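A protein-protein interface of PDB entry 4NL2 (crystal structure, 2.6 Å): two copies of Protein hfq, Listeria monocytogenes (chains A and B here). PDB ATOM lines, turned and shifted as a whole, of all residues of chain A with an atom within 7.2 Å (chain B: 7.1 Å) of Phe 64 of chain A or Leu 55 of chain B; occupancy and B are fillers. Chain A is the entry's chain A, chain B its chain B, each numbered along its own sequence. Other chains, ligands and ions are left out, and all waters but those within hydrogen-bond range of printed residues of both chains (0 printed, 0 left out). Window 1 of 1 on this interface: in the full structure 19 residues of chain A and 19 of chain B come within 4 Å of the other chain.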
ATOM      1  N   LEU A   8      11.803 -14.371  30.131  1.00  0.00           N
ATOM      2  CA  LEU A   8      11.467 -13.010  29.775  1.00  0.00           C
ATOM      3  C   LEU A   8      12.673 -12.348  29.148  1.00  0.00           C
ATOM      4  O   LEU A   8      12.578 -11.736  28.081  1.00  0.00           O
ATOM      5  CB  LEU A   8      11.082 -12.213  31.019  1.00  0.00           C
ATOM      6  CG  LEU A   8      10.060 -11.081  30.944  1.00  0.00           C
ATOM      7  CD1 LEU A   8      10.361 -10.043  32.012  1.00  0.00           C
ATOM      8  CD2 LEU A   8      10.058 -10.441  29.579  1.00  0.00           C
ATOM      9  N   GLN A   9      13.808 -12.508  29.810  1.00  0.00           N
ATOM     10  CA  GLN A   9      15.041 -11.879  29.382  1.00  0.00           C
ATOM     11  C   GLN A   9      15.488 -12.292  27.976  1.00  0.00           C
ATOM     12  O   GLN A   9      15.791 -11.447  27.143  1.00  0.00           O
ATOM     13  CB  GLN A   9      16.134 -12.232  30.384  1.00  0.00           C
ATOM     14  CG  GLN A   9      17.460 -11.601  30.125  1.00  0.00           C
ATOM     15  CD  GLN A   9      18.508 -12.161  31.062  1.00  0.00           C
ATOM     16  OE1 GLN A   9      18.928 -13.301  30.905  1.00  0.00           O
ATOM     17  NE2 GLN A   9      18.901 -11.385  32.069  1.00  0.00           N
ATOM     18  N   ASP A  10      15.531 -13.591  27.721  1.00  0.00           N
ATOM     19  CA  ASP A  10      16.021 -14.089  26.441  1.00  0.00           C
ATOM     20  C   ASP A  10      15.068 -13.778  25.316  1.00  0.00           C
ATOM     21  O   ASP A  10      15.497 -13.485  24.210  1.00  0.00           O
ATOM     22  CB  ASP A  10      16.375 -15.575  26.499  1.00  0.00           C
ATOM     23  CG  ASP A  10      17.587 -15.842  27.375  1.00  0.00           C
ATOM     24  OD1 ASP A  10      18.290 -14.866  27.728  1.00  0.00           O
ATOM     25  OD2 ASP A  10      17.738 -16.979  27.869  1.00  0.00           O
ATOM     26  N   TYR A  12      12.864 -11.219  25.326  1.00  0.00           N
ATOM     27  CA  TYR A  12      12.810  -9.783  25.147  1.00  0.00           C
ATOM     28  C   TYR A  12      13.993  -9.238  24.399  1.00  0.00           C
ATOM     29  O   TYR A  12      13.818  -8.472  23.451  1.00  0.00           O
ATOM     30  CB  TYR A  12      12.672  -9.083  26.498  1.00  0.00           C
ATOM     31  CG  TYR A  12      12.162  -7.663  26.424  1.00  0.00           C
ATOM     32  CD1 TYR A  12      13.029  -6.604  26.249  1.00  0.00           C
ATOM     33  CD2 TYR A  12      10.813  -7.386  26.555  1.00  0.00           C
ATOM     34  CE1 TYR A  12      12.570  -5.316  26.194  1.00  0.00           C
ATOM     35  CE2 TYR A  12      10.343  -6.097  26.505  1.00  0.00           C
ATOM     36  CZ  TYR A  12      11.224  -5.068  26.322  1.00  0.00           C
ATOM     37  OH  TYR A  12      10.767  -3.777  26.272  1.00  0.00           O
ATOM     38  N   LEU A  13      15.195  -9.644  24.810  1.00  0.00           N
ATOM     39  CA  LEU A  13      16.418  -9.144  24.173  1.00  0.00           C
ATOM     40  C   LEU A  13      16.505  -9.679  22.751  1.00  0.00           C
ATOM     41  O   LEU A  13      17.006  -8.998  21.858  1.00  0.00           O
ATOM     42  CB  LEU A  13      17.687  -9.503  24.972  1.00  0.00           C
ATOM     43  CG  LEU A  13      17.820  -8.848  26.353  1.00  0.00           C
ATOM     44  CD1 LEU A  13      19.151  -9.166  27.039  1.00  0.00           C
ATOM     45  CD2 LEU A  13      17.605  -7.348  26.233  1.00  0.00           C
ATOM     46  N   LEU A  16      14.392  -7.504  20.621  1.00  0.00           N
ATOM     47  CA  LEU A  16      15.096  -6.253  20.360  1.00  0.00           C
ATOM     48  C   LEU A  16      16.177  -6.481  19.337  1.00  0.00           C
ATOM     49  O   LEU A  16      16.459  -5.602  18.524  1.00  0.00           O
ATOM     50  CB  LEU A  16      15.739  -5.694  21.630  1.00  0.00           C
ATOM     51  CG  LEU A  16      14.844  -5.103  22.719  1.00  0.00           C
ATOM     52  CD1 LEU A  16      15.665  -4.741  23.957  1.00  0.00           C
ATOM     53  CD2 LEU A  16      14.145  -3.865  22.193  1.00  0.00           C
ATOM     54  N   ALA A  23      17.129   1.513  21.515  1.00  0.00           N
ATOM     55  CA  ALA A  23      16.839   1.536  22.941  1.00  0.00           C
ATOM     56  C   ALA A  23      17.885   2.277  23.714  1.00  0.00           C
ATOM     57  O   ALA A  23      19.046   2.296  23.343  1.00  0.00           O
ATOM     58  CB  ALA A  23      16.729   0.140  23.476  1.00  0.00           C
ATOM     59  N   THR A  24      17.452   2.954  24.765  1.00  0.00           N
ATOM     60  CA  THR A  24      18.389   3.581  25.666  1.00  0.00           C
ATOM     61  C   THR A  24      18.730   2.566  26.750  1.00  0.00           C
ATOM     62  O   THR A  24      17.837   2.055  27.418  1.00  0.00           O
ATOM     63  CB  THR A  24      17.812   4.806  26.365  1.00  0.00           C
ATOM     64  OG1 THR A  24      17.388   5.755  25.398  1.00  0.00           O
ATOM     65  CG2 THR A  24      18.887   5.467  27.219  1.00  0.00           C
ATOM     66  N   VAL A  25      20.011   2.232  26.870  1.00  0.00           N
ATOM     67  CA  VAL A  25      20.498   1.297  27.880  1.00  0.00           C
ATOM     68  C   VAL A  25      21.113   2.046  29.065  1.00  0.00           C
ATOM     69  O   VAL A  25      22.216   2.580  28.978  1.00  0.00           O
ATOM     70  CB  VAL A  25      21.504   0.298  27.308  1.00  0.00           C
ATOM     71  CG1 VAL A  25      21.973  -0.658  28.377  1.00  0.00           C
ATOM     72  CG2 VAL A  25      20.889  -0.441  26.148  1.00  0.00           C
ATOM     73  N   PHE A  26      20.371   2.143  30.153  1.00  0.00           N
ATOM     74  CA  PHE A  26      20.870   2.822  31.339  1.00  0.00           C
ATOM     75  C   PHE A  26      21.795   1.908  32.126  1.00  0.00           C
ATOM     76  O   PHE A  26      21.430   0.811  32.469  1.00  0.00           O
ATOM     77  CB  PHE A  26      19.713   3.273  32.214  1.00  0.00           C
ATOM     78  CG  PHE A  26      18.757   4.200  31.526  1.00  0.00           C
ATOM     79  CD1 PHE A  26      18.978   5.567  31.524  1.00  0.00           C
ATOM     80  CD2 PHE A  26      17.625   3.700  30.888  1.00  0.00           C
ATOM     81  CE1 PHE A  26      18.091   6.420  30.896  1.00  0.00           C
ATOM     82  CE2 PHE A  26      16.736   4.545  30.265  1.00  0.00           C
ATOM     83  CZ  PHE A  26      16.965   5.907  30.265  1.00  0.00           C
ATOM     84  N   GLY A  35      21.392   2.659  21.446  1.00  0.00           N
ATOM     85  CA  GLY A  35      21.744   1.858  20.299  1.00  0.00           C
ATOM     86  C   GLY A  35      20.849   0.666  20.056  1.00  0.00           C
ATOM     87  O   GLY A  35      19.701   0.625  20.516  1.00  0.00           O
ATOM     88  N   ARG A  36      21.387  -0.306  19.322  1.00  0.00           N
ATOM     89  CA  ARG A  36      20.651  -1.494  18.949  1.00  0.00           C
ATOM     90  C   ARG A  36      21.413  -2.754  19.301  1.00  0.00           C
ATOM     91  O   ARG A  36      22.640  -2.754  19.325  1.00  0.00           O
ATOM     92  CB  ARG A  36      20.378  -1.477  17.442  1.00  0.00           C
ATOM     93  CG  ARG A  36      19.436  -0.386  16.995  1.00  0.00           C
ATOM     94  CD  ARG A  36      19.400  -0.250  15.486  1.00  0.00           C
ATOM     95  NE  ARG A  36      18.275   0.591  15.084  1.00  0.00           N
ATOM     96  CZ  ARG A  36      18.315   1.914  15.027  1.00  0.00           C
ATOM     97  NH1 ARG A  36      19.440   2.553  15.322  1.00  0.00           N
ATOM     98  NH2 ARG A  36      17.241   2.594  14.657  1.00  0.00           N
ATOM     99  N   VAL A  37      20.680  -3.829  19.561  1.00  0.00           N
ATOM    100  CA  VAL A  37      21.268  -5.108  19.932  1.00  0.00           C
ATOM    101  C   VAL A  37      21.741  -5.931  18.731  1.00  0.00           C
ATOM    102  O   VAL A  37      20.978  -6.216  17.812  1.00  0.00           O
ATOM    103  CB  VAL A  37      20.295  -5.937  20.799  1.00  0.00           C
ATOM    104  CG1 VAL A  37      20.826  -7.348  21.026  1.00  0.00           C
ATOM    105  CG2 VAL A  37      20.015  -5.217  22.108  1.00  0.00           C
ATOM    106  N   VAL A  45      25.952  -7.959  26.421  1.00  0.00           N
ATOM    107  CA  VAL A  45      25.141  -7.553  25.293  1.00  0.00           C
ATOM    108  C   VAL A  45      26.035  -6.779  24.345  1.00  0.00           C
ATOM    109  O   VAL A  45      26.732  -5.859  24.753  1.00  0.00           O
ATOM    110  CB  VAL A  45      23.980  -6.637  25.700  1.00  0.00           C
ATOM    111  CG1 VAL A  45      23.116  -6.382  24.496  1.00  0.00           C
ATOM    112  CG2 VAL A  45      23.147  -7.270  26.772  1.00  0.00           C
ATOM    113  N   LEU A  47      26.351  -4.242  21.559  1.00  0.00           N
ATOM    114  CA  LEU A  47      25.523  -3.120  21.140  1.00  0.00           C
ATOM    115  C   LEU A  47      26.082  -2.354  19.929  1.00  0.00           C
ATOM    116  O   LEU A  47      27.289  -2.197  19.774  1.00  0.00           O
ATOM    117  CB  LEU A  47      25.361  -2.179  22.325  1.00  0.00           C
ATOM    118  CG  LEU A  47      23.999  -1.871  22.907  1.00  0.00           C
ATOM    119  CD1 LEU A  47      23.148  -3.096  23.032  1.00  0.00           C
ATOM    120  CD2 LEU A  47      24.296  -1.320  24.260  1.00  0.00           C
ATOM    121  N   VAL A  56      28.721  -4.598  26.363  1.00  0.00           N
ATOM    122  CA  VAL A  56      28.292  -4.178  27.688  1.00  0.00           C
ATOM    123  C   VAL A  56      28.019  -5.378  28.583  1.00  0.00           C
ATOM    124  O   VAL A  56      27.284  -6.279  28.195  1.00  0.00           O
ATOM    125  CB  VAL A  56      26.994  -3.393  27.562  1.00  0.00           C
ATOM    126  CG1 VAL A  56      26.575  -2.802  28.883  1.00  0.00           C
ATOM    127  CG2 VAL A  56      27.141  -2.340  26.473  1.00  0.00           C
ATOM    128  N   LYS A  58      26.122  -7.319  31.315  1.00  0.00           N
ATOM    129  CA  LYS A  58      24.750  -7.274  31.814  1.00  0.00           C
ATOM    130  C   LYS A  58      24.643  -6.844  33.272  1.00  0.00           C
ATOM    131  O   LYS A  58      23.678  -6.213  33.658  1.00  0.00           O
ATOM    132  CB  LYS A  58      24.080  -8.617  31.654  1.00  0.00           C
ATOM    133  CG  LYS A  58      23.614  -8.925  30.270  1.00  0.00           C
ATOM    134  CD  LYS A  58      22.872 -10.247  30.330  1.00  0.00           C
ATOM    135  CE  LYS A  58      22.172 -10.623  29.052  1.00  0.00           C
ATOM    136  NZ  LYS A  58      21.540 -11.965  29.311  1.00  0.00           N
ATOM    137  N   ILE A  61      24.200  -3.243  33.569  1.00  0.00           N
ATOM    138  CA  ILE A  61      22.986  -2.692  33.021  1.00  0.00           C
ATOM    139  C   ILE A  61      21.892  -2.555  34.052  1.00  0.00           C
ATOM    140  O   ILE A  61      21.664  -3.443  34.861  1.00  0.00           O
ATOM    141  CB  ILE A  61      22.469  -3.504  31.838  1.00  0.00           C
ATOM    142  CG1 ILE A  61      23.496  -3.467  30.711  1.00  0.00           C
ATOM    143  CG2 ILE A  61      21.124  -2.943  31.368  1.00  0.00           C
ATOM    144  CD1 ILE A  61      23.068  -4.188  29.431  1.00  0.00           C
ATOM    145  N   SER A  62      21.243  -1.405  34.025  1.00  0.00           N
ATOM    146  CA  SER A  62      20.120  -1.127  34.877  1.00  0.00           C
ATOM    147  C   SER A  62      18.794  -1.333  34.119  1.00  0.00           C
ATOM    148  O   SER A  62      17.899  -2.031  34.590  1.00  0.00           O
ATOM    149  CB  SER A  62      20.229   0.301  35.379  1.00  0.00           C
ATOM    150  OG  SER A  62      19.122   0.621  36.175  1.00  0.00           O
ATOM    151  N   THR A  63      18.688  -0.760  32.923  1.00  0.00           N
ATOM    152  CA  THR A  63      17.433  -0.744  32.207  1.00  0.00           C
ATOM    153  C   THR A  63      17.549  -0.671  30.695  1.00  0.00           C
ATOM    154  O   THR A  63      18.387   0.057  30.172  1.00  0.00           O
ATOM    155  CB  THR A  63      16.625   0.512  32.623  1.00  0.00           C
ATOM    156  OG1 THR A  63      16.286   0.438  34.013  1.00  0.00           O
ATOM    157  CG2 THR A  63      15.342   0.628  31.820  1.00  0.00           C
ATOM    158  N   PHE A  64      16.753  -1.475  29.996  1.00  0.00           N
ATOM    159  CA  PHE A  64      16.552  -1.288  28.567  1.00  0.00           C
ATOM    160  C   PHE A  64      15.261  -0.474  28.362  1.00  0.00           C
ATOM    161  O   PHE A  64      14.202  -0.849  28.857  1.00  0.00           O
ATOM    162  CB  PHE A  64      16.424  -2.625  27.854  1.00  0.00           C
ATOM    163  CG  PHE A  64      17.747  -3.268  27.519  1.00  0.00           C
ATOM    164  CD1 PHE A  64      18.389  -4.081  28.445  1.00  0.00           C
ATOM    165  CD2 PHE A  64      18.351  -3.049  26.292  1.00  0.00           C
ATOM    166  CE1 PHE A  64      19.600  -4.665  28.150  1.00  0.00           C
ATOM    167  CE2 PHE A  64      19.559  -3.642  25.992  1.00  0.00           C
ATOM    168  CZ  PHE A  64      20.183  -4.447  26.918  1.00  0.00           C
ATOM    169  N   SER A  65      15.340   0.631  27.635  1.00  0.00           N
ATOM    170  CA  SER A  65      14.168   1.474  27.397  1.00  0.00           C
ATOM    171  C   SER A  65      13.956   1.617  25.871  1.00  0.00           C
ATOM    172  O   SER A  65      14.507   2.514  25.244  1.00  0.00           O
ATOM    173  CB  SER A  65      14.413   2.830  28.068  1.00  0.00           C
ATOM    174  OG  SER A  65      13.297   3.694  27.995  1.00  0.00           O
ATOM    175  N   PRO A  66      13.124   0.740  25.278  1.00  0.00           N
ATOM    176  CA  PRO A  66      12.918   0.700  23.820  1.00  0.00           C
ATOM    177  C   PRO A  66      12.069   1.845  23.286  1.00  0.00           C
ATOM    178  O   PRO A  66      11.219   2.347  24.009  1.00  0.00           O
ATOM    179  CB  PRO A  66      12.200  -0.632  23.614  1.00  0.00           C
ATOM    180  CG  PRO A  66      11.445  -0.833  24.875  1.00  0.00           C
ATOM    181  CD  PRO A  66      12.316  -0.283  25.971  1.00  0.00           C
ATOM    182  N   LEU B  33      11.401   4.366  39.097  1.00  0.00           N
ATOM    183  CA  LEU B  33      10.415   4.315  38.045  1.00  0.00           C
ATOM    184  C   LEU B  33       9.088   4.127  38.733  1.00  0.00           C
ATOM    185  O   LEU B  33       9.005   3.415  39.725  1.00  0.00           O
ATOM    186  CB  LEU B  33      10.652   3.109  37.138  1.00  0.00           C
ATOM    187  CG  LEU B  33      12.017   2.905  36.499  1.00  0.00           C
ATOM    188  CD1 LEU B  33      12.900   2.082  37.412  1.00  0.00           C
ATOM    189  CD2 LEU B  33      11.868   2.190  35.189  1.00  0.00           C
ATOM    190  N   SER B  39       5.602  -8.338  33.596  1.00  0.00           N
ATOM    191  CA  SER B  39       6.135  -9.681  33.648  1.00  0.00           C
ATOM    192  C   SER B  39       7.443  -9.705  34.414  1.00  0.00           C
ATOM    193  O   SER B  39       7.934  -8.661  34.834  1.00  0.00           O
ATOM    194  CB  SER B  39       6.347 -10.180  32.222  1.00  0.00           C
ATOM    195  OG  SER B  39       6.910 -11.475  32.230  1.00  0.00           O
ATOM    196  N   ASP B  41      11.150 -12.543  35.308  1.00  0.00           N
ATOM    197  CA  ASP B  41      11.770 -13.840  35.525  1.00  0.00           C
ATOM    198  C   ASP B  41      12.761 -13.775  36.687  1.00  0.00           C
ATOM    199  O   ASP B  41      12.635 -12.920  37.554  1.00  0.00           O
ATOM    200  CB  ASP B  41      12.378 -14.444  34.257  1.00  0.00           C
ATOM    201  CG  ASP B  41      13.311 -13.510  33.538  1.00  0.00           C
ATOM    202  OD1 ASP B  41      13.787 -12.522  34.143  1.00  0.00           O
ATOM    203  OD2 ASP B  41      13.575 -13.784  32.354  1.00  0.00           O
ATOM    204  N   THR B  44      15.007 -10.421  35.445  1.00  0.00           N
ATOM    205  CA  THR B  44      14.439  -9.191  34.925  1.00  0.00           C
ATOM    206  C   THR B  44      13.002  -8.967  35.329  1.00  0.00           C
ATOM    207  O   THR B  44      12.284  -9.912  35.649  1.00  0.00           O
ATOM    208  CB  THR B  44      14.518  -9.163  33.400  1.00  0.00           C
ATOM    209  OG1 THR B  44      13.934 -10.367  32.907  1.00  0.00           O
ATOM    210  CG2 THR B  44      15.948  -9.150  32.958  1.00  0.00           C
ATOM    211  N   VAL B  45      12.594  -7.704  35.308  1.00  0.00           N
ATOM    212  CA  VAL B  45      11.204  -7.343  35.515  1.00  0.00           C
ATOM    213  C   VAL B  45      10.801  -6.403  34.384  1.00  0.00           C
ATOM    214  O   VAL B  45      11.449  -5.386  34.164  1.00  0.00           O
ATOM    215  CB  VAL B  45      11.021  -6.550  36.814  1.00  0.00           C
ATOM    216  CG1 VAL B  45       9.557  -6.304  37.040  1.00  0.00           C
ATOM    217  CG2 VAL B  45      11.572  -7.309  37.960  1.00  0.00           C
ATOM    218  N   LEU B  46       9.754  -6.749  33.650  1.00  0.00           N
ATOM    219  CA  LEU B  46       9.245  -5.883  32.596  1.00  0.00           C
ATOM    220  C   LEU B  46       8.225  -4.925  33.168  1.00  0.00           C
ATOM    221  O   LEU B  46       7.225  -5.337  33.746  1.00  0.00           O
ATOM    222  CB  LEU B  46       8.635  -6.701  31.461  1.00  0.00           C
ATOM    223  CG  LEU B  46       8.094  -5.918  30.266  1.00  0.00           C
ATOM    224  CD1 LEU B  46       9.155  -4.997  29.732  1.00  0.00           C
ATOM    225  CD2 LEU B  46       7.670  -6.888  29.180  1.00  0.00           C
ATOM    226  N   LEU B  47       8.468  -3.638  33.010  1.00  0.00           N
ATOM    227  CA  LEU B  47       7.613  -2.626  33.615  1.00  0.00           C
ATOM    228  C   LEU B  47       6.815  -1.793  32.628  1.00  0.00           C
ATOM    229  O   LEU B  47       7.281  -1.534  31.522  1.00  0.00           O
ATOM    230  CB  LEU B  47       8.483  -1.689  34.437  1.00  0.00           C
ATOM    231  CG  LEU B  47       8.271  -1.636  35.933  1.00  0.00           C
ATOM    232  CD1 LEU B  47       8.428  -3.003  36.491  1.00  0.00           C
ATOM    233  CD2 LEU B  47       9.346  -0.729  36.484  1.00  0.00           C
ATOM    234  N   LYS B  52       4.905   3.055  28.215  1.00  0.00           N
ATOM    235  CA  LYS B  52       6.173   2.553  27.685  1.00  0.00           C
ATOM    236  C   LYS B  52       6.796   1.402  28.492  1.00  0.00           C
ATOM    237  O   LYS B  52       6.789   1.401  29.732  1.00  0.00           O
ATOM    238  CB  LYS B  52       7.179   3.689  27.454  1.00  0.00           C
ATOM    239  CG  LYS B  52       8.411   3.257  26.655  1.00  0.00           C
ATOM    240  CD  LYS B  52       9.721   3.721  27.288  1.00  0.00           C
ATOM    241  CE  LYS B  52      10.106   5.130  26.831  1.00  0.00           C
ATOM    242  NZ  LYS B  52       9.185   6.178  27.348  1.00  0.00           N
ATOM    243  N   GLN B  53       7.316   0.413  27.773  1.00  0.00           N
ATOM    244  CA  GLN B  53       7.971  -0.723  28.400  1.00  0.00           C
ATOM    245  C   GLN B  53       9.355  -0.356  28.907  1.00  0.00           C
ATOM    246  O   GLN B  53      10.079   0.443  28.304  1.00  0.00           O
ATOM    247  CB  GLN B  53       8.075  -1.902  27.446  1.00  0.00           C
ATOM    248  CG  GLN B  53       6.776  -2.584  27.143  1.00  0.00           C
ATOM    249  CD  GLN B  53       6.973  -3.714  26.178  1.00  0.00           C
ATOM    250  OE1 GLN B  53       8.000  -3.795  25.510  1.00  0.00           O
ATOM    251  NE2 GLN B  53       5.991  -4.588  26.080  1.00  0.00           N
ATOM    252  N   GLN B  54       9.713  -0.970  30.024  1.00  0.00           N
ATOM    253  CA  GLN B  54      10.997  -0.762  30.672  1.00  0.00           C
ATOM    254  C   GLN B  54      11.509  -2.093  31.202  1.00  0.00           C
ATOM    255  O   GLN B  54      11.016  -2.600  32.199  1.00  0.00           O
ATOM    256  CB  GLN B  54      10.847   0.245  31.825  1.00  0.00           C
ATOM    257  CG  GLN B  54      11.792   1.405  31.739  1.00  0.00           C
ATOM    258  CD  GLN B  54      11.318   2.510  30.808  1.00  0.00           C
ATOM    259  OE1 GLN B  54      12.127   3.301  30.297  1.00  0.00           O
ATOM    260  NE2 GLN B  54      10.011   2.595  30.610  1.00  0.00           N
ATOM    261  N   LEU B  55      12.421  -2.715  30.481  1.00  0.00           N
ATOM    262  CA  LEU B  55      12.994  -3.967  30.956  1.00  0.00           C
ATOM    263  C   LEU B  55      14.059  -3.661  32.034  1.00  0.00           C
ATOM    264  O   LEU B  55      15.110  -3.112  31.738  1.00  0.00           O
ATOM    265  CB  LEU B  55      13.573  -4.791  29.804  1.00  0.00           C
ATOM    266  CG  LEU B  55      14.037  -6.167  30.264  1.00  0.00           C
ATOM    267  CD1 LEU B  55      12.841  -7.030  30.656  1.00  0.00           C
ATOM    268  CD2 LEU B  55      14.894  -6.841  29.226  1.00  0.00           C
ATOM    269  N   VAL B  56      13.772  -4.003  33.281  1.00  0.00           N
ATOM    270  CA  VAL B  56      14.660  -3.673  34.390  1.00  0.00           C
ATOM    271  C   VAL B  56      15.361  -4.895  34.977  1.00  0.00           C
ATOM    272  O   VAL B  56      14.714  -5.885  35.322  1.00  0.00           O
ATOM    273  CB  VAL B  56      13.872  -2.957  35.521  1.00  0.00           C
ATOM    274  CG1 VAL B  56      14.790  -2.555  36.668  1.00  0.00           C
ATOM    275  CG2 VAL B  56      13.122  -1.783  34.979  1.00  0.00           C
ATOM    276  N   PHE B  57      16.680  -4.839  35.093  1.00  0.00           N
ATOM    277  CA  PHE B  57      17.381  -5.945  35.730  1.00  0.00           C
ATOM    278  C   PHE B  57      17.189  -5.944  37.237  1.00  0.00           C
ATOM    279  O   PHE B  57      17.356  -4.918  37.898  1.00  0.00           O
ATOM    280  CB  PHE B  57      18.868  -5.908  35.398  1.00  0.00           C
ATOM    281  CG  PHE B  57      19.190  -6.497  34.057  1.00  0.00           C
ATOM    282  CD1 PHE B  57      19.280  -7.865  33.900  1.00  0.00           C
ATOM    283  CD2 PHE B  57      19.341  -5.691  32.939  1.00  0.00           C
ATOM    284  CE1 PHE B  57      19.542  -8.420  32.662  1.00  0.00           C
ATOM    285  CE2 PHE B  57      19.598  -6.242  31.708  1.00  0.00           C
ATOM    286  CZ  PHE B  57      19.706  -7.604  31.569  1.00  0.00           C
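The backbone NH (N) of Phe 64 of chain A lies within hydrogen-bond range of the backbone carbonyl oxygen (O) of Leu 55 of chain B (2.9 Å). The side-chain amide oxygen of Gln 54 of chain B sits at hydrogen-bond distance from the side-chain hydroxyl of Ser 65 of chain A (2.6 Å). N of Leu 8 of chain A is in hydrogen-bond range of OD2 of Asp 41 of chain B. N of Gln 9 of chain A is in hydrogen-bond range of OD2 of Asp 41 of chain B (2.9 Å). The side-chain hydroxyl of Tyr 12 of chain A lies within hydrogen-bond range of the side-chain amide oxygen of Gln 53 of chain B (2.9 Å). The backbone carbonyl oxygen (O) of Ser 62 of chain A is in hydrogen-bond range of the backbone NH (N) of Phe 57 of chain B (3.1 Å).
O of Val 56 of chain B sits at hydrogen-bond distance from N of Val 45 of chain B (2.8 Å). The backbone NH (N) of Leu 47 of chain B lies within hydrogen-bond range of the backbone carbonyl oxygen (O) of Gln 54 of chain B. O of Ser 39 of chain B is in hydrogen-bond range of N of Leu 46 of chain B. The side-chain amino group (NZ) of Lys 58 of chain A lies within hydrogen-bond range of the side-chain amide oxygen (OE1) of Gln 9 of chain A (3.3 Å). The backbone carbonyl oxygen (O) of Phe 26 of chain A sits at hydrogen-bond distance from the backbone NH (N) of Ser 62 of chain A, at 2.7 Å. The backbone NH of Ser 65 of chain A lies within hydrogen-bond range of the backbone carbonyl oxygen of Thr 24 of chain A, at 2.9 Å.
CG of Leu 8 of chain A touches OG of Ser 39 of chain B, at 3.4 Å. OG1 of Thr 44 of chain B touches CD1 of Leu 8 of chain A, at 3.7 Å. Thr 44 of chain B touches Gln 9 of chain A. NE2 of Gln 9 of chain A touches CE1 of Phe 57 of chain B, at 3.1 Å. CG2 of Ile 61 of chain A touches CD2 of Phe 57 of chain B, at 3.6 Å. O of Ser 62 of chain A touches CA of Val 56 of chain B, 3.6 Å away. OG1 of Thr 63 of chain A touches CG2 of Val 56 of chain B, 3.98 Å away. Ser 65 of chain A touches Lys 52 of chain B (OG to CD, 3.6 Å). Pro 66 of chain A touches Lys 52 of chain B. Gln 53 of chain B touches Pro 66 of chain A (O to CD, 3.3 Å).
Val 56 of chain A touches none of the printed residues of chain B. Lys 58 of chain A touches none of the printed residues of chain B. Of the printed residues of chain B, Ile 61 of chain A touches Phe 57. Of the printed residues of chain B, Ser 62 of chain A touches Val 56 (3.6 Å) and Phe 57 (3.1 Å). Of chain B, only Gln 54 (3.7 Å), Leu 55 (2.9 Å) and Phe 57 (3.9 Å) come within 4 Å of Phe 64 of chain A. Of the printed residues of chain B, Pro 66 of chain A touches Lys 52 (3.9 Å) and Gln 53 (3.3 Å). Of the printed residues of chain A, Asp 41 of chain B touches Leu 8 (2.9 Å) and Gln 9 (2.9 Å). Of the printed residues of chain A, Leu 55 of chain B touches Tyr 12 (3.5 Å), Thr 63 (3.4 Å) and Phe 64 (2.9 Å). The nearest residue of chain A that does not touch Leu 55 of chain B is Leu 13 of chain A (4.1 Å). The nearest printed residue of chain A that does not touch Thr 44 of chain B is Asp 10 of chain A (6.3 Å).
Hydrophobic or aromatic side chains of chain A that line the printed part of chain B: Leu 8, Tyr 12, Ile 61, Phe 64 and Pro 66. Hydrophobic or aromatic side chains of chain B that line the printed part of chain A: Leu 46, Leu 55, Val 56 and Phe 57.
3 positions are printed for both chains. Of the 23 pairs that touch across the chains among the printed residues, none has its exchanged pair printed and touching as well.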
